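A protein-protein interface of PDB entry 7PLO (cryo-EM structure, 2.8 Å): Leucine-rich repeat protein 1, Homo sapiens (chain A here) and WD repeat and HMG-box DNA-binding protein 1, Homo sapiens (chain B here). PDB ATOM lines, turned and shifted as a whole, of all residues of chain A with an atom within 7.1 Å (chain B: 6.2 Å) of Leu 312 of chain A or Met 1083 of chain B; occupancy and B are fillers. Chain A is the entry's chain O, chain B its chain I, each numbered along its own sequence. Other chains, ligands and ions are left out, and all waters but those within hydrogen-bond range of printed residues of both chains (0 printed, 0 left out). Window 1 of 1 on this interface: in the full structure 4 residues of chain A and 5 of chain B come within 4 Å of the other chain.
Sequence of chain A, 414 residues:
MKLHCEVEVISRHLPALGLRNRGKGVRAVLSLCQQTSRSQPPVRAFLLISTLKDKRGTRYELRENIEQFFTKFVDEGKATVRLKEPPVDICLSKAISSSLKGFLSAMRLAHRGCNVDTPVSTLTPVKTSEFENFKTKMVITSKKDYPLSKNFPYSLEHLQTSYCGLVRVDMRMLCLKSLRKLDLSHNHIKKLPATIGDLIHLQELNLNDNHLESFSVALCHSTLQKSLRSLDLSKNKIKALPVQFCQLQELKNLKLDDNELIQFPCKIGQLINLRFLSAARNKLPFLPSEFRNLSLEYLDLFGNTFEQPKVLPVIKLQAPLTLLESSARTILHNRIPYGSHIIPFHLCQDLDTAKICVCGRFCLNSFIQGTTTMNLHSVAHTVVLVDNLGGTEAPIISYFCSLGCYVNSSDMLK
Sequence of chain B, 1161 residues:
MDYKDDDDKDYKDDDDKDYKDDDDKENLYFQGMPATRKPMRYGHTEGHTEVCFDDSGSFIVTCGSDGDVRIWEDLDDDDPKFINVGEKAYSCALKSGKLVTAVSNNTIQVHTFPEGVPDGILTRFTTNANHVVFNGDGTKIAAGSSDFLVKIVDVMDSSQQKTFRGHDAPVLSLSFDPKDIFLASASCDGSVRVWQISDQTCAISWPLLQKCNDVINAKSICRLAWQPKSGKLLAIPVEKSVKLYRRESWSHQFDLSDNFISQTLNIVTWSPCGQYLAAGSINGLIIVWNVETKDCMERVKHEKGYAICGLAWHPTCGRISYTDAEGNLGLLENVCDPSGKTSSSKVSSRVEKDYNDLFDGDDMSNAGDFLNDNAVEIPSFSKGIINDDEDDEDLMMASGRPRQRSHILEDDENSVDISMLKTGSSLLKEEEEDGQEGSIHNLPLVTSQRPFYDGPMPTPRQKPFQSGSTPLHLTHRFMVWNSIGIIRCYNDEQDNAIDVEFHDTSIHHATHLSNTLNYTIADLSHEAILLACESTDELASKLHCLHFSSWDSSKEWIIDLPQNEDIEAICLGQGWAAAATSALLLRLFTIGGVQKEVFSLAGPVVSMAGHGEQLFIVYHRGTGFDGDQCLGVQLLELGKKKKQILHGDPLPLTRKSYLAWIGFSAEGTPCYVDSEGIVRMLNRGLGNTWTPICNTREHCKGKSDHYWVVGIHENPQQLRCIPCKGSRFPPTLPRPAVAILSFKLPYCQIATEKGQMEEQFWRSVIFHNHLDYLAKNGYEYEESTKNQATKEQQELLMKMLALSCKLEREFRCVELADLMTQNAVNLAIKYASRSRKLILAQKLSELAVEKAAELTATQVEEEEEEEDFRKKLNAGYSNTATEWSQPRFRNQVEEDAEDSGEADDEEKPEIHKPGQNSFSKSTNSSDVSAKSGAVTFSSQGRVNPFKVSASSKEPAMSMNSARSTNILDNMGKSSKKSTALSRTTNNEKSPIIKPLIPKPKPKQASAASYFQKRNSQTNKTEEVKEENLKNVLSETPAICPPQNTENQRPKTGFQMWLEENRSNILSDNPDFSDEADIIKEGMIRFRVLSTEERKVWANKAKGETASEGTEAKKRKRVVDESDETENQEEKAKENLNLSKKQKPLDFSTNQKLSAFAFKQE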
ATOM      1  N   PRO A 309       6.776  10.846 -33.076  1.00  0.00           N
ATOM      2  CA  PRO A 309       5.924  11.108 -31.909  1.00  0.00           C
ATOM      3  C   PRO A 309       4.446  11.194 -32.256  1.00  0.00           C
ATOM      4  O   PRO A 309       4.052  11.493 -33.386  1.00  0.00           O
ATOM      5  CB  PRO A 309       6.441  12.452 -31.393  1.00  0.00           C
ATOM      6  CG  PRO A 309       6.810  13.160 -32.616  1.00  0.00           C
ATOM      7  CD  PRO A 309       7.384  12.112 -33.540  1.00  0.00           C
ATOM      8  N   LYS A 310       3.625  10.923 -31.238  1.00  0.00           N
ATOM      9  CA  LYS A 310       2.176  11.071 -31.304  1.00  0.00           C
ATOM     10  C   LYS A 310       1.708  12.384 -30.683  1.00  0.00           C
ATOM     11  O   LYS A 310       0.621  12.443 -30.096  1.00  0.00           O
ATOM     12  CB  LYS A 310       1.495   9.889 -30.615  1.00  0.00           C
ATOM     13  N   VAL A 311       2.513  13.441 -30.800  1.00  0.00           N
ATOM     14  CA  VAL A 311       2.183  14.747 -30.239  1.00  0.00           C
ATOM     15  C   VAL A 311       0.962  15.303 -30.957  1.00  0.00           C
ATOM     16  O   VAL A 311       0.581  14.807 -32.023  1.00  0.00           O
ATOM     17  CB  VAL A 311       3.373  15.717 -30.344  1.00  0.00           C
ATOM     18  N   LEU A 312       0.350  16.344 -30.385  1.00  0.00           N
ATOM     19  CA  LEU A 312      -0.913  16.901 -30.870  1.00  0.00           C
ATOM     20  C   LEU A 312      -0.792  18.415 -31.047  1.00  0.00           C
ATOM     21  O   LEU A 312      -1.381  19.192 -30.285  1.00  0.00           O
ATOM     22  CB  LEU A 312      -2.048  16.543 -29.906  1.00  0.00           C
ATOM     23  CG  LEU A 312      -3.488  16.758 -30.382  1.00  0.00           C
ATOM     24  CD1 LEU A 312      -3.843  15.836 -31.539  1.00  0.00           C
ATOM     25  CD2 LEU A 312      -4.477  16.551 -29.256  1.00  0.00           C
ATOM     26  N   PRO A 313      -0.028  18.874 -32.064  1.00  0.00           N
ATOM     27  CA  PRO A 313       0.033  20.318 -32.390  1.00  0.00           C
ATOM     28  C   PRO A 313      -1.044  20.720 -33.396  1.00  0.00           C
ATOM     29  O   PRO A 313      -0.777  21.054 -34.559  1.00  0.00           O
ATOM     30  CB  PRO A 313       1.445  20.456 -32.956  1.00  0.00           C
ATOM     31  CG  PRO A 313       1.619  19.183 -33.718  1.00  0.00           C
ATOM     32  CD  PRO A 313       0.916  18.110 -32.901  1.00  0.00           C
ATOM     33  N   VAL A 314      -2.293  20.696 -32.951  1.00  0.00           N
ATOM     34  CA  VAL A 314      -3.426  20.841 -33.859  1.00  0.00           C
ATOM     35  C   VAL A 314      -3.637  22.313 -34.176  1.00  0.00           C
ATOM     36  O   VAL A 314      -3.527  23.178 -33.297  1.00  0.00           O
ATOM     37  CB  VAL A 314      -4.694  20.210 -33.249  1.00  0.00           C
ATOM     38  CG1 VAL A 314      -5.933  20.510 -34.101  1.00  0.00           C
ATOM     39  CG2 VAL A 314      -4.532  18.706 -33.112  1.00  0.00           C
ATOM     40  N   ILE A 315      -3.950  22.602 -35.439  1.00  0.00           N
ATOM     41  CA  ILE A 315      -4.337  23.957 -35.830  1.00  0.00           C
ATOM     42  C   ILE A 315      -5.817  24.144 -35.524  1.00  0.00           C
ATOM     43  O   ILE A 315      -6.643  23.284 -35.849  1.00  0.00           O
ATOM     44  CB  ILE A 315      -4.031  24.216 -37.317  1.00  0.00           C
ATOM     45  CG1 ILE A 315      -2.511  24.246 -37.545  1.00  0.00           C
ATOM     46  CG2 ILE A 315      -4.688  25.539 -37.784  1.00  0.00           C
ATOM     47  CD1 ILE A 315      -2.075  24.187 -39.006  1.00  0.00           C
ATOM     48  N   LYS A 316      -6.154  25.272 -34.902  1.00  0.00           N
ATOM     49  CA  LYS A 316      -7.520  25.583 -34.503  1.00  0.00           C
ATOM     50  C   LYS A 316      -8.205  26.447 -35.558  1.00  0.00           C
ATOM     51  O   LYS A 316      -7.560  27.167 -36.324  1.00  0.00           O
ATOM     52  CB  LYS A 316      -7.537  26.289 -33.145  1.00  0.00           C
ATOM     53  CG  LYS A 316      -7.620  25.342 -31.942  1.00  0.00           C
ATOM     54  CD  LYS A 316      -6.410  24.414 -31.780  1.00  0.00           C
ATOM     55  CE  LYS A 316      -5.177  25.180 -31.336  1.00  0.00           C
ATOM     56  NZ  LYS A 316      -4.015  24.319 -30.997  1.00  0.00           N
ATOM     57  N   GLN A 369      -6.374  20.806 -38.554  1.00  0.00           N
ATOM     58  CA  GLN A 369      -5.375  19.871 -39.053  1.00  0.00           C
ATOM     59  C   GLN A 369      -4.538  19.290 -37.920  1.00  0.00           C
ATOM     60  O   GLN A 369      -4.144  20.009 -36.989  1.00  0.00           O
ATOM     61  CB  GLN A 369      -4.459  20.562 -40.067  1.00  0.00           C
ATOM     62  CG  GLN A 369      -3.387  19.663 -40.663  1.00  0.00           C
ATOM     63  CD  GLN A 369      -2.756  20.267 -41.903  1.00  0.00           C
ATOM     64  OE1 GLN A 369      -3.448  20.591 -42.868  1.00  0.00           O
ATOM     65  NE2 GLN A 369      -1.438  20.429 -41.880  1.00  0.00           N
ATOM     66  N   GLY A 370      -4.273  17.987 -38.024  1.00  0.00           N
ATOM     67  CA  GLY A 370      -3.370  17.275 -37.133  1.00  0.00           C
ATOM     68  C   GLY A 370      -2.731  16.112 -37.879  1.00  0.00           C
ATOM     69  O   GLY A 370      -2.566  16.162 -39.102  1.00  0.00           O
ATOM     70  N   THR A 371      -2.410  15.039 -37.150  1.00  0.00           N
ATOM     71  CA  THR A 371      -1.718  13.900 -37.744  1.00  0.00           C
ATOM     72  C   THR A 371      -2.012  12.637 -36.943  1.00  0.00           C
ATOM     73  O   THR A 371      -2.100  12.683 -35.712  1.00  0.00           O
ATOM     74  CB  THR A 371      -0.203  14.171 -37.818  1.00  0.00           C
ATOM     75  OG1 THR A 371       0.061  15.100 -38.878  1.00  0.00           O
ATOM     76  CG2 THR A 371       0.616  12.893 -38.057  1.00  0.00           C
ATOM     77  N   PHE A 400      -9.587  16.599 -37.349  1.00  0.00           N
ATOM     78  CA  PHE A 400      -9.972  16.197 -35.994  1.00  0.00           C
ATOM     79  C   PHE A 400     -11.237  16.913 -35.531  1.00  0.00           C
ATOM     80  O   PHE A 400     -11.278  17.536 -34.466  1.00  0.00           O
ATOM     81  CB  PHE A 400      -8.828  16.467 -35.009  1.00  0.00           C
ATOM     82  CG  PHE A 400      -7.619  15.554 -35.150  1.00  0.00           C
ATOM     83  CD1 PHE A 400      -7.672  14.317 -35.786  1.00  0.00           C
ATOM     84  CD2 PHE A 400      -6.418  15.949 -34.598  1.00  0.00           C
ATOM     85  CE1 PHE A 400      -6.552  13.520 -35.876  1.00  0.00           C
ATOM     86  CE2 PHE A 400      -5.296  15.156 -34.687  1.00  0.00           C
ATOM     87  CZ  PHE A 400      -5.363  13.941 -35.325  1.00  0.00           C
ATOM     88  N   GLY A 404     -12.631  12.559 -33.976  1.00  0.00           N
ATOM     89  CA  GLY A 404     -11.245  12.521 -34.416  1.00  0.00           C
ATOM     90  C   GLY A 404     -10.302  13.173 -33.421  1.00  0.00           C
ATOM     91  O   GLY A 404      -9.230  12.640 -33.124  1.00  0.00           O
ATOM     92  N   CYS A 405     -10.692  14.333 -32.884  1.00  0.00           N
ATOM     93  CA  CYS A 405      -9.889  14.978 -31.849  1.00  0.00           C
ATOM     94  C   CYS A 405      -9.847  14.134 -30.585  1.00  0.00           C
ATOM     95  O   CYS A 405      -8.820  14.075 -29.899  1.00  0.00           O
ATOM     96  CB  CYS A 405     -10.445  16.370 -31.547  1.00  0.00           C
ATOM     97  N   TYR A 406     -10.963  13.483 -30.258  1.00  0.00           N
ATOM     98  CA  TYR A 406     -10.980  12.583 -29.105  1.00  0.00           C
ATOM     99  C   TYR A 406      -9.995  11.432 -29.290  1.00  0.00           C
ATOM    100  O   TYR A 406      -9.246  11.083 -28.367  1.00  0.00           O
ATOM    101  CB  TYR A 406     -12.394  12.048 -28.879  1.00  0.00           C
ATOM    102  N   VAL A 407      -9.966  10.844 -30.488  1.00  0.00           N
ATOM    103  CA  VAL A 407      -9.044   9.746 -30.767  1.00  0.00           C
ATOM    104  C   VAL A 407      -7.603  10.240 -30.744  1.00  0.00           C
ATOM    105  O   VAL A 407      -6.698   9.532 -30.286  1.00  0.00           O
ATOM    106  CB  VAL A 407      -9.394   9.090 -32.113  1.00  0.00           C
ATOM    107  N   ASN A 408      -7.362  11.451 -31.251  1.00  0.00           N
ATOM    108  CA  ASN A 408      -6.017  12.017 -31.206  1.00  0.00           C
ATOM    109  C   ASN A 408      -5.562  12.241 -29.768  1.00  0.00           C
ATOM    110  O   ASN A 408      -4.397  11.997 -29.433  1.00  0.00           O
ATOM    111  CB  ASN A 408      -5.978  13.329 -31.987  1.00  0.00           C
ATOM    112  N   SER A 409      -6.465  12.718 -28.909  1.00  0.00           N
ATOM    113  CA  SER A 409      -6.136  12.875 -27.496  1.00  0.00           C
ATOM    114  C   SER A 409      -5.840  11.527 -26.853  1.00  0.00           C
ATOM    115  O   SER A 409      -4.933  11.413 -26.019  1.00  0.00           O
ATOM    116  CB  SER A 409      -7.281  13.577 -26.767  1.00  0.00           C
ATOM    117  N   SER A 410      -6.601  10.494 -27.223  1.00  0.00           N
ATOM    118  CA  SER A 410      -6.327   9.155 -26.712  1.00  0.00           C
ATOM    119  C   SER A 410      -4.960   8.658 -27.172  1.00  0.00           C
ATOM    120  O   SER A 410      -4.249   7.981 -26.420  1.00  0.00           O
ATOM    121  CB  SER A 410      -7.424   8.189 -27.161  1.00  0.00           C
ATOM    122  N   MET A 412      -2.298  10.562 -28.040  1.00  0.00           N
ATOM    123  CA  MET A 412      -1.224  11.380 -27.484  1.00  0.00           C
ATOM    124  C   MET A 412      -0.888  10.955 -26.058  1.00  0.00           C
ATOM    125  O   MET A 412       0.156  11.322 -25.518  1.00  0.00           O
ATOM    126  CB  MET A 412      -1.613  12.859 -27.509  1.00  0.00           C
ATOM    127  N   PHE B1054     -15.191  17.456 -23.988  1.00  0.00           N
ATOM    128  CA  PHE B1054     -14.055  18.361 -23.857  1.00  0.00           C
ATOM    129  C   PHE B1054     -14.471  19.806 -24.100  1.00  0.00           C
ATOM    130  O   PHE B1054     -14.044  20.710 -23.375  1.00  0.00           O
ATOM    131  CB  PHE B1054     -12.941  17.964 -24.826  1.00  0.00           C
ATOM    132  CG  PHE B1054     -11.872  19.011 -24.970  1.00  0.00           C
ATOM    133  CD1 PHE B1054     -11.167  19.453 -23.862  1.00  0.00           C
ATOM    134  CD2 PHE B1054     -11.573  19.555 -26.209  1.00  0.00           C
ATOM    135  CE1 PHE B1054     -10.188  20.419 -23.985  1.00  0.00           C
ATOM    136  CE2 PHE B1054     -10.592  20.521 -26.338  1.00  0.00           C
ATOM    137  CZ  PHE B1054      -9.900  20.953 -25.223  1.00  0.00           C
ATOM    138  N   TRP B1057     -16.403  21.062 -21.069  1.00  0.00           N
ATOM    139  CA  TRP B1057     -15.460  21.395 -20.004  1.00  0.00           C
ATOM    140  C   TRP B1057     -14.764  22.720 -20.292  1.00  0.00           C
ATOM    141  O   TRP B1057     -14.599  23.558 -19.396  1.00  0.00           O
ATOM    142  CB  TRP B1057     -14.427  20.270 -19.828  1.00  0.00           C
ATOM    143  CG  TRP B1057     -13.339  20.627 -18.834  1.00  0.00           C
ATOM    144  CD1 TRP B1057     -13.325  20.361 -17.497  1.00  0.00           C
ATOM    145  CD2 TRP B1057     -12.117  21.325 -19.115  1.00  0.00           C
ATOM    146  NE1 TRP B1057     -12.176  20.858 -16.927  1.00  0.00           N
ATOM    147  CE2 TRP B1057     -11.423  21.460 -17.901  1.00  0.00           C
ATOM    148  CE3 TRP B1057     -11.560  21.869 -20.275  1.00  0.00           C
ATOM    149  CZ2 TRP B1057     -10.193  22.100 -17.819  1.00  0.00           C
ATOM    150  CZ3 TRP B1057     -10.349  22.505 -20.192  1.00  0.00           C
ATOM    151  CH2 TRP B1057      -9.679  22.620 -18.976  1.00  0.00           C
ATOM    152  N   LEU B1058     -14.312  22.908 -21.533  1.00  0.00           N
ATOM    153  CA  LEU B1058     -13.576  24.118 -21.880  1.00  0.00           C
ATOM    154  C   LEU B1058     -14.460  25.349 -21.761  1.00  0.00           C
ATOM    155  O   LEU B1058     -14.003  26.410 -21.321  1.00  0.00           O
ATOM    156  CB  LEU B1058     -13.010  23.990 -23.296  1.00  0.00           C
ATOM    157  CG  LEU B1058     -12.236  25.178 -23.876  1.00  0.00           C
ATOM    158  CD1 LEU B1058     -11.021  25.524 -23.027  1.00  0.00           C
ATOM    159  CD2 LEU B1058     -11.823  24.873 -25.305  1.00  0.00           C
ATOM    160  N   ILE B1078      -5.779  29.054 -25.889  1.00  0.00           N
ATOM    161  CA  ILE B1078      -6.757  28.717 -24.859  1.00  0.00           C
ATOM    162  C   ILE B1078      -7.204  27.264 -25.009  1.00  0.00           C
ATOM    163  O   ILE B1078      -7.270  26.519 -24.024  1.00  0.00           O
ATOM    164  CB  ILE B1078      -7.931  29.717 -24.918  1.00  0.00           C
ATOM    165  CG1 ILE B1078      -7.471  31.080 -24.381  1.00  0.00           C
ATOM    166  CG2 ILE B1078      -9.136  29.231 -24.111  1.00  0.00           C
ATOM    167  CD1 ILE B1078      -8.254  32.263 -24.908  1.00  0.00           C
ATOM    168  N   ILE B1079      -7.485  26.833 -26.244  1.00  0.00           N
ATOM    169  CA  ILE B1079      -7.838  25.433 -26.496  1.00  0.00           C
ATOM    170  C   ILE B1079      -6.678  24.515 -26.117  1.00  0.00           C
ATOM    171  O   ILE B1079      -6.877  23.412 -25.598  1.00  0.00           O
ATOM    172  CB  ILE B1079      -8.262  25.257 -27.972  1.00  0.00           C
ATOM    173  CG1 ILE B1079      -9.657  25.868 -28.190  1.00  0.00           C
ATOM    174  CG2 ILE B1079      -8.237  23.772 -28.395  1.00  0.00           C
ATOM    175  CD1 ILE B1079     -10.031  26.162 -29.645  1.00  0.00           C
ATOM    176  N   LYS B1080      -5.451  24.963 -26.374  1.00  0.00           N
ATOM    177  CA  LYS B1080      -4.244  24.185 -26.099  1.00  0.00           C
ATOM    178  C   LYS B1080      -4.056  23.948 -24.595  1.00  0.00           C
ATOM    179  O   LYS B1080      -3.897  22.801 -24.136  1.00  0.00           O
ATOM    180  CB  LYS B1080      -3.095  24.980 -26.723  1.00  0.00           C
ATOM    181  CG  LYS B1080      -1.662  24.483 -26.737  1.00  0.00           C
ATOM    182  CD  LYS B1080      -0.876  25.577 -27.500  1.00  0.00           C
ATOM    183  CE  LYS B1080       0.622  25.413 -27.564  1.00  0.00           C
ATOM    184  NZ  LYS B1080       1.191  26.669 -28.150  1.00  0.00           N
ATOM    185  N   GLU B1081      -4.105  25.029 -23.812  1.00  0.00           N
ATOM    186  CA  GLU B1081      -4.035  24.923 -22.356  1.00  0.00           C
ATOM    187  C   GLU B1081      -5.196  24.095 -21.811  1.00  0.00           C
ATOM    188  O   GLU B1081      -5.025  23.300 -20.870  1.00  0.00           O
ATOM    189  CB  GLU B1081      -4.022  26.338 -21.759  1.00  0.00           C
ATOM    190  CG  GLU B1081      -4.072  26.462 -20.230  1.00  0.00           C
ATOM    191  CD  GLU B1081      -2.831  25.931 -19.541  1.00  0.00           C
ATOM    192  OE1 GLU B1081      -1.866  25.561 -20.241  1.00  0.00           O
ATOM    193  OE2 GLU B1081      -2.820  25.893 -18.293  1.00  0.00           O
ATOM    194  N   GLY B1082      -6.389  24.273 -22.387  1.00  0.00           N
ATOM    195  CA  GLY B1082      -7.529  23.476 -21.971  1.00  0.00           C
ATOM    196  C   GLY B1082      -7.325  21.994 -22.219  1.00  0.00           C
ATOM    197  O   GLY B1082      -7.731  21.163 -21.407  1.00  0.00           O
ATOM    198  N   MET B1083      -6.702  21.645 -23.348  1.00  0.00           N
ATOM    199  CA  MET B1083      -6.399  20.244 -23.621  1.00  0.00           C
ATOM    200  C   MET B1083      -5.442  19.681 -22.580  1.00  0.00           C
ATOM    201  O   MET B1083      -5.611  18.542 -22.125  1.00  0.00           O
ATOM    202  CB  MET B1083      -5.813  20.084 -25.028  1.00  0.00           C
ATOM    203  CG  MET B1083      -6.855  19.908 -26.132  1.00  0.00           C
ATOM    204  SD  MET B1083      -6.177  19.199 -27.644  1.00  0.00           S
ATOM    205  CE  MET B1083      -7.678  18.712 -28.496  1.00  0.00           C
ATOM    206  N   ILE B1084      -4.441  20.473 -22.179  1.00  0.00           N
ATOM    207  CA  ILE B1084      -3.497  20.012 -21.152  1.00  0.00           C
ATOM    208  C   ILE B1084      -4.233  19.709 -19.840  1.00  0.00           C
ATOM    209  O   ILE B1084      -4.094  18.621 -19.250  1.00  0.00           O
ATOM    210  CB  ILE B1084      -2.373  21.054 -20.959  1.00  0.00           C
ATOM    211  CG1 ILE B1084      -1.472  21.106 -22.208  1.00  0.00           C
ATOM    212  CG2 ILE B1084      -1.534  20.740 -19.707  1.00  0.00           C
ATOM    213  CD1 ILE B1084      -0.585  22.350 -22.326  1.00  0.00           C
ATOM    214  N   ARG B1085      -5.055  20.657 -19.381  1.00  0.00           N
ATOM    215  CA  ARG B1085      -5.781  20.463 -18.121  1.00  0.00           C
ATOM    216  C   ARG B1085      -6.771  19.293 -18.212  1.00  0.00           C
ATOM    217  O   ARG B1085      -6.884  18.468 -17.281  1.00  0.00           O
ATOM    218  CB  ARG B1085      -6.493  21.766 -17.753  1.00  0.00           C
ATOM    219  CG  ARG B1085      -5.552  22.934 -17.437  1.00  0.00           C
ATOM    220  CD  ARG B1085      -6.284  24.269 -17.245  1.00  0.00           C
ATOM    221  NE  ARG B1085      -5.322  25.359 -17.073  1.00  0.00           N
ATOM    222  CZ  ARG B1085      -5.353  26.314 -16.145  1.00  0.00           C
ATOM    223  NH1 ARG B1085      -6.367  26.452 -15.302  1.00  0.00           N
ATOM    224  NH2 ARG B1085      -4.336  27.170 -16.069  1.00  0.00           N
ATOM    225  N   PHE B1086      -7.491  19.199 -19.335  1.00  0.00           N
ATOM    226  CA  PHE B1086      -8.454  18.123 -19.534  1.00  0.00           C
ATOM    227  C   PHE B1086      -7.771  16.764 -19.569  1.00  0.00           C
ATOM    228  O   PHE B1086      -8.382  15.754 -19.198  1.00  0.00           O
ATOM    229  CB  PHE B1086      -9.232  18.374 -20.828  1.00  0.00           C
ATOM    230  CG  PHE B1086     -10.421  17.476 -21.014  1.00  0.00           C
ATOM    231  CD1 PHE B1086     -11.592  17.699 -20.309  1.00  0.00           C
ATOM    232  CD2 PHE B1086     -10.378  16.423 -21.912  1.00  0.00           C
ATOM    233  CE1 PHE B1086     -12.691  16.878 -20.481  1.00  0.00           C
ATOM    234  CE2 PHE B1086     -11.474  15.599 -22.091  1.00  0.00           C
ATOM    235  CZ  PHE B1086     -12.632  15.828 -21.375  1.00  0.00           C
ATOM    236  N   ARG B1087      -6.513  16.712 -20.013  1.00  0.00           N
ATOM    237  CA  ARG B1087      -5.754  15.473 -19.891  1.00  0.00           C
ATOM    238  C   ARG B1087      -5.390  15.177 -18.446  1.00  0.00           C
ATOM    239  O   ARG B1087      -5.309  14.005 -18.058  1.00  0.00           O
ATOM    240  CB  ARG B1087      -4.483  15.538 -20.727  1.00  0.00           C
ATOM    241  CG  ARG B1087      -4.719  15.387 -22.202  1.00  0.00           C
ATOM    242  CD  ARG B1087      -3.429  15.561 -22.953  1.00  0.00           C
ATOM    243  NE  ARG B1087      -3.654  15.656 -24.388  1.00  0.00           N
ATOM    244  CZ  ARG B1087      -2.699  15.761 -25.301  1.00  0.00           C
ATOM    245  NH1 ARG B1087      -1.414  15.767 -24.977  1.00  0.00           N
ATOM    246  NH2 ARG B1087      -3.041  15.862 -26.580  1.00  0.00           N
ATOM    247  N   VAL B1088      -5.147  16.214 -17.639  1.00  0.00           N
ATOM    248  CA  VAL B1088      -4.793  15.944 -16.244  1.00  0.00           C
ATOM    249  C   VAL B1088      -5.987  15.403 -15.455  1.00  0.00           C
ATOM    250  O   VAL B1088      -5.784  14.729 -14.437  1.00  0.00           O
ATOM    251  CB  VAL B1088      -4.191  17.201 -15.576  1.00  0.00           C
ATOM    252  CG1 VAL B1088      -3.886  16.975 -14.070  1.00  0.00           C
ATOM    253  CG2 VAL B1088      -2.906  17.606 -16.295  1.00  0.00           C
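The backbone carbonyl oxygen (O) of Val 314 of chain A is in hydrogen-bond range of the side-chain amino group (NZ) of Lys 316 of chain A (2.6 Å).
Among the printed residues, pairs that only touch across the chains: Leu 312 of chain A with Met 1083 of chain B (3.5 Å), Leu 312 of chain A with Arg 1087 of chain B (3.1 Å), Lys 316 of chain A with Ile 1079 of chain B (3.4 Å) and Met 412 of chain A with Arg 1087 of chain B (3.5 Å).
Leu 312 of chain A touches two residues of chain B.
Printed residues of chain A within 4 Å of Met 1083 of chain B: Leu 312.
No residue of chain A comes within 4 Å of Gly 1082 of chain B.
Printed residues of chain A within 4 Å of Arg 1087 of chain B: Leu 312 (3.1 Å) and Met 412 (3.5 Å).
Printed residues of chain A within 4 Å of Ile 1079 of chain B: Lys 316.
Of the printed residues of chain B, Met 412 of chain A touches Arg 1087.
Printed residues of chain B within 4 Å of Lys 316 of chain A: Ile 1079.
The nearest residue of chain A that does not touch Met 1083 of chain B is Cys 405 of chain A (4.7 Å).
Of the 20 printed residues of chain A, 3 touch a printed residue of chain B.
Hydrophobic or aromatic side chains of chain A within 4 Å of the printed part of chain B: Leu 312 and Met 412.
Along chain A the printed residues that touch a printed residue of chain B span positions 312 to 412.
Of the 14 printed residues of chain B, 3 touch a printed residue of chain A.
Printed residues of chain B that touch a printed residue of chain A: Ile 1079, Met 1083 and Arg 1087.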
